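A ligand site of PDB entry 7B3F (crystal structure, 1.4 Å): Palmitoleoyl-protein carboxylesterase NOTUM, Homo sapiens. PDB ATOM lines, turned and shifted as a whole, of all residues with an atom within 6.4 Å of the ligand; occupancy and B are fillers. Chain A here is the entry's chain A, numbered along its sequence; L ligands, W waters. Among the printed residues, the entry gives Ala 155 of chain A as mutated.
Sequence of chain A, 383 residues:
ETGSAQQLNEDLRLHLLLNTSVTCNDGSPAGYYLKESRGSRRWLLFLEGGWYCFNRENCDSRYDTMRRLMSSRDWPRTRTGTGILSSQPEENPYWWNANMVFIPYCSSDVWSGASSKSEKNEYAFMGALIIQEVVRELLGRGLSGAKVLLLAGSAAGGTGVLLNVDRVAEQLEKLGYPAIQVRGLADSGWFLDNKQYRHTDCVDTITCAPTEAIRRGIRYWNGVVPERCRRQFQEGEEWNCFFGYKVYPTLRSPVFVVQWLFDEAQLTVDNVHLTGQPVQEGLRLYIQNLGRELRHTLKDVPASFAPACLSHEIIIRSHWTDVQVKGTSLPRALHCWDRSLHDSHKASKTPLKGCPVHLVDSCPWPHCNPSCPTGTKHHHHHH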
ATOM      1  N   GLY A  49       9.714 -20.028  -7.137  1.00  0.00           N
ATOM      2  CA  GLY A  49      10.053 -19.149  -6.049  1.00  0.00           C
ATOM      3  C   GLY A  49       8.960 -19.071  -5.001  1.00  0.00           C
ATOM      4  O   GLY A  49       8.041 -19.912  -4.943  1.00  0.00           O
ATOM      5  N   GLY A  50       9.049 -18.038  -4.154  1.00  0.00           N
ATOM      6  CA  GLY A  50       8.101 -17.860  -3.076  1.00  0.00           C
ATOM      7  C   GLY A  50       8.740 -17.574  -1.732  1.00  0.00           C
ATOM      8  O   GLY A  50       8.446 -18.269  -0.749  1.00  0.00           O
ATOM      9  N   TRP A  51       9.590 -16.552  -1.632  1.00  0.00           N
ATOM     10  CA  TRP A  51      10.166 -16.124  -0.329  1.00  0.00           C
ATOM     11  C   TRP A  51      10.989 -17.270   0.278  1.00  0.00           C
ATOM     12  O   TRP A  51      11.681 -17.993  -0.456  1.00  0.00           O
ATOM     13  CB  TRP A  51       9.117 -15.510   0.594  1.00  0.00           C
ATOM     14  CG  TRP A  51       8.578 -14.232   0.048  1.00  0.00           C
ATOM     15  CD1 TRP A  51       7.493 -14.088  -0.736  1.00  0.00           C
ATOM     16  CD2 TRP A  51       9.152 -12.938   0.214  1.00  0.00           C
ATOM     17  NE1 TRP A  51       7.307 -12.754  -1.058  1.00  0.00           N
ATOM     18  CE2 TRP A  51       8.324 -12.027  -0.484  1.00  0.00           C
ATOM     19  CE3 TRP A  51      10.278 -12.452   0.889  1.00  0.00           C
ATOM     20  CZ2 TRP A  51       8.588 -10.649  -0.528  1.00  0.00           C
ATOM     21  CZ3 TRP A  51      10.559 -11.078   0.830  1.00  0.00           C
ATOM     22  CH2 TRP A  51       9.693 -10.192   0.144  1.00  0.00           C
ATOM     23  N   TYR A  52      10.953 -17.405   1.605  1.00  0.00           N
ATOM     24  CA  TYR A  52      11.881 -18.258   2.356  1.00  0.00           C
ATOM     25  C   TYR A  52      11.420 -18.158   3.815  1.00  0.00           C
ATOM     26  O   TYR A  52      10.576 -17.334   4.148  1.00  0.00           O
ATOM     27  CB  TYR A  52      13.354 -17.815   2.260  1.00  0.00           C
ATOM     28  CG  TYR A  52      13.528 -16.306   2.363  1.00  0.00           C
ATOM     29  CD1 TYR A  52      13.493 -15.662   3.592  1.00  0.00           C
ATOM     30  CD2 TYR A  52      13.763 -15.536   1.221  1.00  0.00           C
ATOM     31  CE1 TYR A  52      13.642 -14.294   3.689  1.00  0.00           C
ATOM     32  CE2 TYR A  52      13.932 -14.159   1.324  1.00  0.00           C
ATOM     33  CZ  TYR A  52      13.847 -13.543   2.538  1.00  0.00           C
ATOM     34  OH  TYR A  52      14.022 -12.172   2.601  1.00  0.00           O
ATOM     35  N   TYR A 105       9.289 -25.534  -5.316  1.00  0.00           N
ATOM     36  CA  TYR A 105      10.073 -24.976  -4.236  1.00  0.00           C
ATOM     37  C   TYR A 105       9.426 -25.416  -2.931  1.00  0.00           C
ATOM     38  O   TYR A 105       8.373 -24.909  -2.549  1.00  0.00           O
ATOM     39  CB  TYR A 105      10.044 -23.463  -4.394  1.00  0.00           C
ATOM     40  CG  TYR A 105      10.810 -22.661  -3.399  1.00  0.00           C
ATOM     41  CD1 TYR A 105      12.093 -23.059  -2.980  1.00  0.00           C
ATOM     42  CD2 TYR A 105      10.304 -21.450  -2.953  1.00  0.00           C
ATOM     43  CE1 TYR A 105      12.838 -22.270  -2.090  1.00  0.00           C
ATOM     44  CE2 TYR A 105      11.044 -20.652  -2.077  1.00  0.00           C
ATOM     45  CZ  TYR A 105      12.290 -21.066  -1.649  1.00  0.00           C
ATOM     46  OH  TYR A 105      12.980 -20.226  -0.803  1.00  0.00           O
ATOM     47  N   VAL A 110      15.838 -20.516  -0.551  1.00  0.00           N
ATOM     48  CA  VAL A 110      16.321 -19.856  -1.778  1.00  0.00           C
ATOM     49  C   VAL A 110      17.171 -20.875  -2.556  1.00  0.00           C
ATOM     50  O   VAL A 110      18.129 -20.532  -3.243  1.00  0.00           O
ATOM     51  CB  VAL A 110      17.081 -18.550  -1.461  1.00  0.00           C
ATOM     52  CG1 VAL A 110      17.280 -17.704  -2.741  1.00  0.00           C
ATOM     53  CG2 VAL A 110      16.388 -17.738  -0.382  1.00  0.00           C
ATOM     54  N   SER A 154      12.120 -18.297 -11.332  1.00  0.00           N
ATOM     55  CA  SER A 154      11.527 -16.993 -11.081  1.00  0.00           C
ATOM     56  C   SER A 154      11.507 -16.711  -9.593  1.00  0.00           C
ATOM     57  O   SER A 154      11.353 -17.613  -8.756  1.00  0.00           O
ATOM     58  CB  SER A 154      10.089 -16.935 -11.579  1.00  0.00           C
ATOM     59  OG  SER A 154      10.024 -17.054 -12.979  1.00  0.00           O
ATOM     60  N   ALA A 155      11.619 -15.438  -9.263  1.00  0.00           N
ATOM     61  CA  ALA A 155      11.516 -14.967  -7.866  1.00  0.00           C
ATOM     62  C   ALA A 155      12.653 -15.623  -7.076  1.00  0.00           C
ATOM     63  O   ALA A 155      13.806 -15.583  -7.538  1.00  0.00           O
ATOM     64  CB  ALA A 155      10.094 -15.215  -7.357  1.00  0.00           C
ATOM     65  N   ALA A 156      12.413 -16.215  -5.903  1.00  0.00           N
ATOM     66  CA  ALA A 156      13.500 -16.899  -5.205  1.00  0.00           C
ATOM     67  C   ALA A 156      14.129 -17.998  -6.060  1.00  0.00           C
ATOM     68  O   ALA A 156      15.301 -18.345  -5.861  1.00  0.00           O
ATOM     69  CB  ALA A 156      12.995 -17.491  -3.868  1.00  0.00           C
ATOM     70  N   GLY A 157      13.380 -18.542  -7.018  1.00  0.00           N
ATOM     71  CA  GLY A 157      13.949 -19.503  -7.946  1.00  0.00           C
ATOM     72  C   GLY A 157      14.944 -18.886  -8.898  1.00  0.00           C
ATOM     73  O   GLY A 157      15.885 -19.543  -9.342  1.00  0.00           O
ATOM     74  N   THR A 159      16.995 -16.389  -7.966  1.00  0.00           N
ATOM     75  CA  THR A 159      18.204 -16.410  -7.152  1.00  0.00           C
ATOM     76  C   THR A 159      18.787 -17.810  -7.082  1.00  0.00           C
ATOM     77  O   THR A 159      20.001 -17.988  -7.171  1.00  0.00           O
ATOM     78  CB  THR A 159      17.904 -15.887  -5.747  1.00  0.00           C
ATOM     79  OG1 THR A 159      17.105 -14.695  -5.869  1.00  0.00           O
ATOM     80  CG2 THR A 159      19.159 -15.537  -5.005  1.00  0.00           C
ATOM     81  N   SER A 188      13.736 -12.289 -11.960  1.00  0.00           N
ATOM     82  CA  SER A 188      13.158 -11.676 -10.764  1.00  0.00           C
ATOM     83  C   SER A 188      13.832 -12.174  -9.481  1.00  0.00           C
ATOM     84  O   SER A 188      13.201 -12.181  -8.402  1.00  0.00           O
ATOM     85  CB  SER A 188      11.639 -11.867 -10.712  1.00  0.00           C
ATOM     86  OG  SER A 188      11.061 -11.219 -11.872  1.00  0.00           O
ATOM     87  N   GLY A 189      15.103 -12.565  -9.595  1.00  0.00           N
ATOM     88  CA  GLY A 189      15.882 -12.917  -8.417  1.00  0.00           C
ATOM     89  C   GLY A 189      17.162 -12.112  -8.252  1.00  0.00           C
ATOM     90  O   GLY A 189      18.084 -12.569  -7.577  1.00  0.00           O
ATOM     91  N   PHE A 191      18.436  -9.056  -6.658  1.00  0.00           N
ATOM     92  CA  PHE A 191      18.058  -8.109  -5.616  1.00  0.00           C
ATOM     93  C   PHE A 191      19.239  -7.247  -5.185  1.00  0.00           C
ATOM     94  O   PHE A 191      20.396  -7.614  -5.362  1.00  0.00           O
ATOM     95  CB  PHE A 191      17.458  -8.841  -4.402  1.00  0.00           C
ATOM     96  CG  PHE A 191      16.246  -9.659  -4.756  1.00  0.00           C
ATOM     97  CD1 PHE A 191      15.064  -9.021  -5.133  1.00  0.00           C
ATOM     98  CD2 PHE A 191      16.280 -11.052  -4.749  1.00  0.00           C
ATOM     99  CE1 PHE A 191      13.933  -9.732  -5.461  1.00  0.00           C
ATOM    100  CE2 PHE A 191      15.157 -11.797  -5.101  1.00  0.00           C
ATOM    101  CZ  PHE A 191      13.967 -11.142  -5.430  1.00  0.00           C
ATOM    102  N   LEU A 192      18.934  -6.104  -4.576  1.00  0.00           N
ATOM    103  CA  LEU A 192      19.952  -5.180  -4.114  1.00  0.00           C
ATOM    104  C   LEU A 192      19.924  -5.107  -2.602  1.00  0.00           C
ATOM    105  O   LEU A 192      18.846  -5.033  -1.998  1.00  0.00           O
ATOM    106  CB  LEU A 192      19.690  -3.768  -4.658  1.00  0.00           C
ATOM    107  CG  LEU A 192      19.590  -3.616  -6.177  1.00  0.00           C
ATOM    108  CD1 LEU A 192      19.399  -2.153  -6.524  1.00  0.00           C
ATOM    109  CD2 LEU A 192      20.865  -4.164  -6.832  1.00  0.00           C
ATOM    110  N   PRO A 210      16.722  -8.126   4.265  1.00  0.00           N
ATOM    111  CA  PRO A 210      17.232  -9.354   3.626  1.00  0.00           C
ATOM    112  C   PRO A 210      18.659  -9.718   3.967  1.00  0.00           C
ATOM    113  O   PRO A 210      18.944 -10.914   4.118  1.00  0.00           O
ATOM    114  CB  PRO A 210      17.106  -9.044   2.133  1.00  0.00           C
ATOM    115  CG  PRO A 210      15.954  -8.176   2.045  1.00  0.00           C
ATOM    116  CD  PRO A 210      15.935  -7.316   3.307  1.00  0.00           C
ATOM    117  N   THR A 211      19.581  -8.749   4.096  1.00  0.00           N
ATOM    118  CA  THR A 211      20.953  -9.135   4.384  1.00  0.00           C
ATOM    119  C   THR A 211      21.006  -9.880   5.696  1.00  0.00           C
ATOM    120  O   THR A 211      21.703 -10.888   5.819  1.00  0.00           O
ATOM    121  CB  THR A 211      21.916  -7.934   4.466  1.00  0.00           C
ATOM    122  OG1 THR A 211      21.394  -6.945   5.341  1.00  0.00           O
ATOM    123  CG2 THR A 211      22.128  -7.318   3.079  1.00  0.00           C
ATOM    124  N   ILE A 214      18.960 -13.355   5.396  1.00  0.00           N
ATOM    125  CA  ILE A 214      19.792 -14.315   4.665  1.00  0.00           C
ATOM    126  C   ILE A 214      20.992 -14.757   5.508  1.00  0.00           C
ATOM    127  O   ILE A 214      21.383 -15.926   5.490  1.00  0.00           O
ATOM    128  CB  ILE A 214      20.227 -13.738   3.312  1.00  0.00           C
ATOM    129  CG1 ILE A 214      19.033 -13.587   2.350  1.00  0.00           C
ATOM    130  CG2 ILE A 214      21.285 -14.641   2.644  1.00  0.00           C
ATOM    131  CD1 ILE A 214      18.268 -14.853   2.099  1.00  0.00           C
ATOM    132  N   PHE A 242      24.094 -14.242  -2.281  1.00  0.00           N
ATOM    133  CA  PHE A 242      22.692 -14.291  -2.646  1.00  0.00           C
ATOM    134  C   PHE A 242      22.237 -13.050  -3.392  1.00  0.00           C
ATOM    135  O   PHE A 242      21.080 -12.969  -3.810  1.00  0.00           O
ATOM    136  CB  PHE A 242      21.863 -14.401  -1.366  1.00  0.00           C
ATOM    137  CG  PHE A 242      21.821 -15.785  -0.768  1.00  0.00           C
ATOM    138  CD1 PHE A 242      22.963 -16.384  -0.217  1.00  0.00           C
ATOM    139  CD2 PHE A 242      20.595 -16.445  -0.662  1.00  0.00           C
ATOM    140  CE1 PHE A 242      22.890 -17.658   0.338  1.00  0.00           C
ATOM    141  CE2 PHE A 242      20.528 -17.709  -0.095  1.00  0.00           C
ATOM    142  CZ  PHE A 242      21.655 -18.302   0.416  1.00  0.00           C
ATOM    143  N   PHE A 243      23.151 -12.105  -3.581  1.00  0.00           N
ATOM    144  CA  PHE A 243      22.866 -10.862  -4.268  1.00  0.00           C
ATOM    145  C   PHE A 243      23.462 -10.926  -5.656  1.00  0.00           C
ATOM    146  O   PHE A 243      24.675 -11.043  -5.812  1.00  0.00           O
ATOM    147  CB  PHE A 243      23.363  -9.688  -3.420  1.00  0.00           C
ATOM    148  CG  PHE A 243      22.510  -9.490  -2.207  1.00  0.00           C
ATOM    149  CD1 PHE A 243      21.374  -8.691  -2.265  1.00  0.00           C
ATOM    150  CD2 PHE A 243      22.750 -10.216  -1.052  1.00  0.00           C
ATOM    151  CE1 PHE A 243      20.541  -8.582  -1.159  1.00  0.00           C
ATOM    152  CE2 PHE A 243      21.916 -10.109   0.032  1.00  0.00           C
ATOM    153  CZ  PHE A 243      20.805  -9.324  -0.035  1.00  0.00           C
ATOM    154  N   ASP A 263      11.190  -3.818  -9.024  1.00  0.00           N
ATOM    155  CA  ASP A 263      10.659  -5.101  -8.647  1.00  0.00           C
ATOM    156  C   ASP A 263       9.853  -5.018  -7.350  1.00  0.00           C
ATOM    157  O   ASP A 263      10.271  -4.359  -6.396  1.00  0.00           O
ATOM    158  CB  ASP A 263      11.807  -6.090  -8.483  1.00  0.00           C
ATOM    159  CG  ASP A 263      11.307  -7.458  -8.111  1.00  0.00           C
ATOM    160  OD1 ASP A 263      10.880  -8.219  -9.005  1.00  0.00           O
ATOM    161  OD2 ASP A 263      11.291  -7.763  -6.897  1.00  0.00           O
ATOM    162  N   ALA A 265       9.033  -7.281  -5.057  1.00  0.00           N
ATOM    163  CA  ALA A 265       9.629  -7.874  -3.855  1.00  0.00           C
ATOM    164  C   ALA A 265      10.772  -6.995  -3.333  1.00  0.00           C
ATOM    165  O   ALA A 265      10.927  -6.820  -2.115  1.00  0.00           O
ATOM    166  CB  ALA A 265      10.117  -9.293  -4.128  1.00  0.00           C
ATOM    167  N   GLN A 266      11.581  -6.455  -4.238  1.00  0.00           N
ATOM    168  CA  GLN A 266      12.589  -5.475  -3.823  1.00  0.00           C
ATOM    169  C   GLN A 266      11.962  -4.310  -3.068  1.00  0.00           C
ATOM    170  O   GLN A 266      12.438  -3.924  -1.996  1.00  0.00           O
ATOM    171  CB  GLN A 266      13.329  -4.967  -5.081  1.00  0.00           C
ATOM    172  CG  GLN A 266      14.369  -3.909  -4.733  1.00  0.00           C
ATOM    173  CD  GLN A 266      15.625  -4.549  -4.171  1.00  0.00           C
ATOM    174  OE1 GLN A 266      16.169  -5.499  -4.759  1.00  0.00           O
ATOM    175  NE2 GLN A 266      16.094  -4.029  -3.018  1.00  0.00           N
ATOM    176  N   VAL A 269      10.909  -5.448   0.482  1.00  0.00           N
ATOM    177  CA  VAL A 269      12.000  -5.517   1.442  1.00  0.00           C
ATOM    178  C   VAL A 269      12.601  -4.159   1.728  1.00  0.00           C
ATOM    179  O   VAL A 269      13.267  -3.991   2.764  1.00  0.00           O
ATOM    180  CB  VAL A 269      13.068  -6.580   1.092  1.00  0.00           C
ATOM    181  CG1 VAL A 269      12.419  -7.931   0.971  1.00  0.00           C
ATOM    182  CG2 VAL A 269      13.827  -6.217  -0.175  1.00  0.00           C
ATOM    183  N   HIS A 312       6.627  -8.418 -10.581  1.00  0.00           N
ATOM    184  CA  HIS A 312       7.505  -9.462 -10.069  1.00  0.00           C
ATOM    185  C   HIS A 312       7.192 -10.743 -10.821  1.00  0.00           C
ATOM    186  O   HIS A 312       6.030 -11.140 -10.890  1.00  0.00           O
ATOM    187  CB  HIS A 312       7.254  -9.690  -8.550  1.00  0.00           C
ATOM    188  CG  HIS A 312       8.310 -10.525  -7.870  1.00  0.00           C
ATOM    189  ND1 HIS A 312       9.666 -10.242  -7.963  1.00  0.00           N
ATOM    190  CD2 HIS A 312       8.217 -11.621  -7.071  1.00  0.00           C
ATOM    191  CE1 HIS A 312      10.353 -11.128  -7.263  1.00  0.00           C
ATOM    192  NE2 HIS A 312       9.503 -11.967  -6.704  1.00  0.00           N
ATOM    193  N   GLU A 313       8.235 -11.372 -11.348  1.00  0.00           N
ATOM    194  CA  GLU A 313       8.194 -12.583 -12.198  1.00  0.00           C
ATOM    195  C   GLU A 313       7.742 -12.279 -13.616  1.00  0.00           C
ATOM    196  O   GLU A 313       6.978 -11.338 -13.843  1.00  0.00           O
ATOM    197  CB  GLU A 313       7.298 -13.656 -11.604  1.00  0.00           C
ATOM    198  CG  GLU A 313       7.761 -14.150 -10.234  1.00  0.00           C
ATOM    199  CD  GLU A 313       6.927 -15.305  -9.743  1.00  0.00           C
ATOM    200  OE1 GLU A 313       5.690 -15.256  -9.870  1.00  0.00           O
ATOM    201  OE2 GLU A 313       7.521 -16.319  -9.376  1.00  0.00           O
HETATM  202  C1  LIG L   1      10.600 -14.043  -3.990  1.00  0.00           C
HETATM  203  C2  LIG L   1      10.369 -13.225  -2.742  1.00  0.00           C
HETATM  204  C3  LIG L   1      11.524 -12.270  -2.394  1.00  0.00           C
HETATM  205  C4  LIG L   1      12.871 -12.941  -2.206  1.00  0.00           C
HETATM  206  C5  LIG L   1      13.858 -10.635  -1.757  1.00  0.00           C
HETATM  207  C6  LIG L   1      15.156 -10.147  -1.154  1.00  0.00           C
HETATM  208  C7  LIG L   1      16.159 -11.266  -1.378  1.00  0.00           C
HETATM  209  C8  LIG L   1      17.531 -11.245  -1.229  1.00  0.00           C
HETATM  210  C9  LIG L   1      18.210 -12.425  -1.544  1.00  0.00           C
HETATM  211  C10 LIG L   1      17.514 -13.573  -1.919  1.00  0.00           C
HETATM  212  C11 LIG L   1      16.132 -13.580  -2.041  1.00  0.00           C
HETATM  213  C12 LIG L   1      15.423 -12.418  -1.736  1.00  0.00           C
HETATM  214  N1  LIG L   1      13.995 -12.097  -1.872  1.00  0.00           N
HETATM  215  O1  LIG L   1      11.085 -13.443  -4.997  1.00  0.00           O
HETATM  216  O2  LIG L   1      10.321 -15.278  -4.022  1.00  0.00           O
HETATM  217  O3  LIG L   1      12.999 -14.125  -2.298  1.00  0.00           O
HETATM  218  O   HOH W   1       7.491 -14.626  -5.075  1.00  0.00           O
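Tyr 52 touches the ligand (CE2 to O3, 3.7 Å). Ala 155 touches the ligand (CB to O1, 3.1 Å). Phe 191 touches the ligand (CD2 to C7, 3.4 Å). Pro 210 touches the ligand. Phe 242 touches the ligand. Phe 243 touches the ligand (CZ to C8, 3.98 Å). Ala 265 touches the ligand. Hydrophobic or aromatic side chains within 4 Å of the ligand: Trp 51, Tyr 52, Ala 155, Ala 156, Phe 191, Pro 210, Phe 243, Ala 265 and His 312. Within 4 Å of the ligand: Gly 50, Trp 51, Tyr 52, Ala 155, Ala 156, Phe 191, Pro 210, Phe 242, Phe 243, Ala 265 and His 312.
A ring nitrogen (ND1) of His 312 lies within hydrogen-bond range of the side-chain carboxylate (OD1) of Asp 263 (2.6 Å). The side-chain hydroxyl of Tyr 105 sits at hydrogen-bond distance from the backbone carbonyl oxygen of Trp 51, 2.6 Å away. The side-chain carboxylate (OD2) of Asp 263 is in hydrogen-bond range of the backbone NH (N) of Ala 265 (3.0 Å).
NE2 of His 312 lies within hydrogen-bond range of O1 of the ligand (2.8 Å). O2 of the ligand is in hydrogen-bond range of N of Trp 51. The backbone NH (N) of Ala 156 is in hydrogen-bond range of an oxygen (O2) of the ligand, 3.0 Å away. The backbone NH (N) of Gly 50 sits at hydrogen-bond distance from an oxygen (O2) of the ligand, 3.0 Å away.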
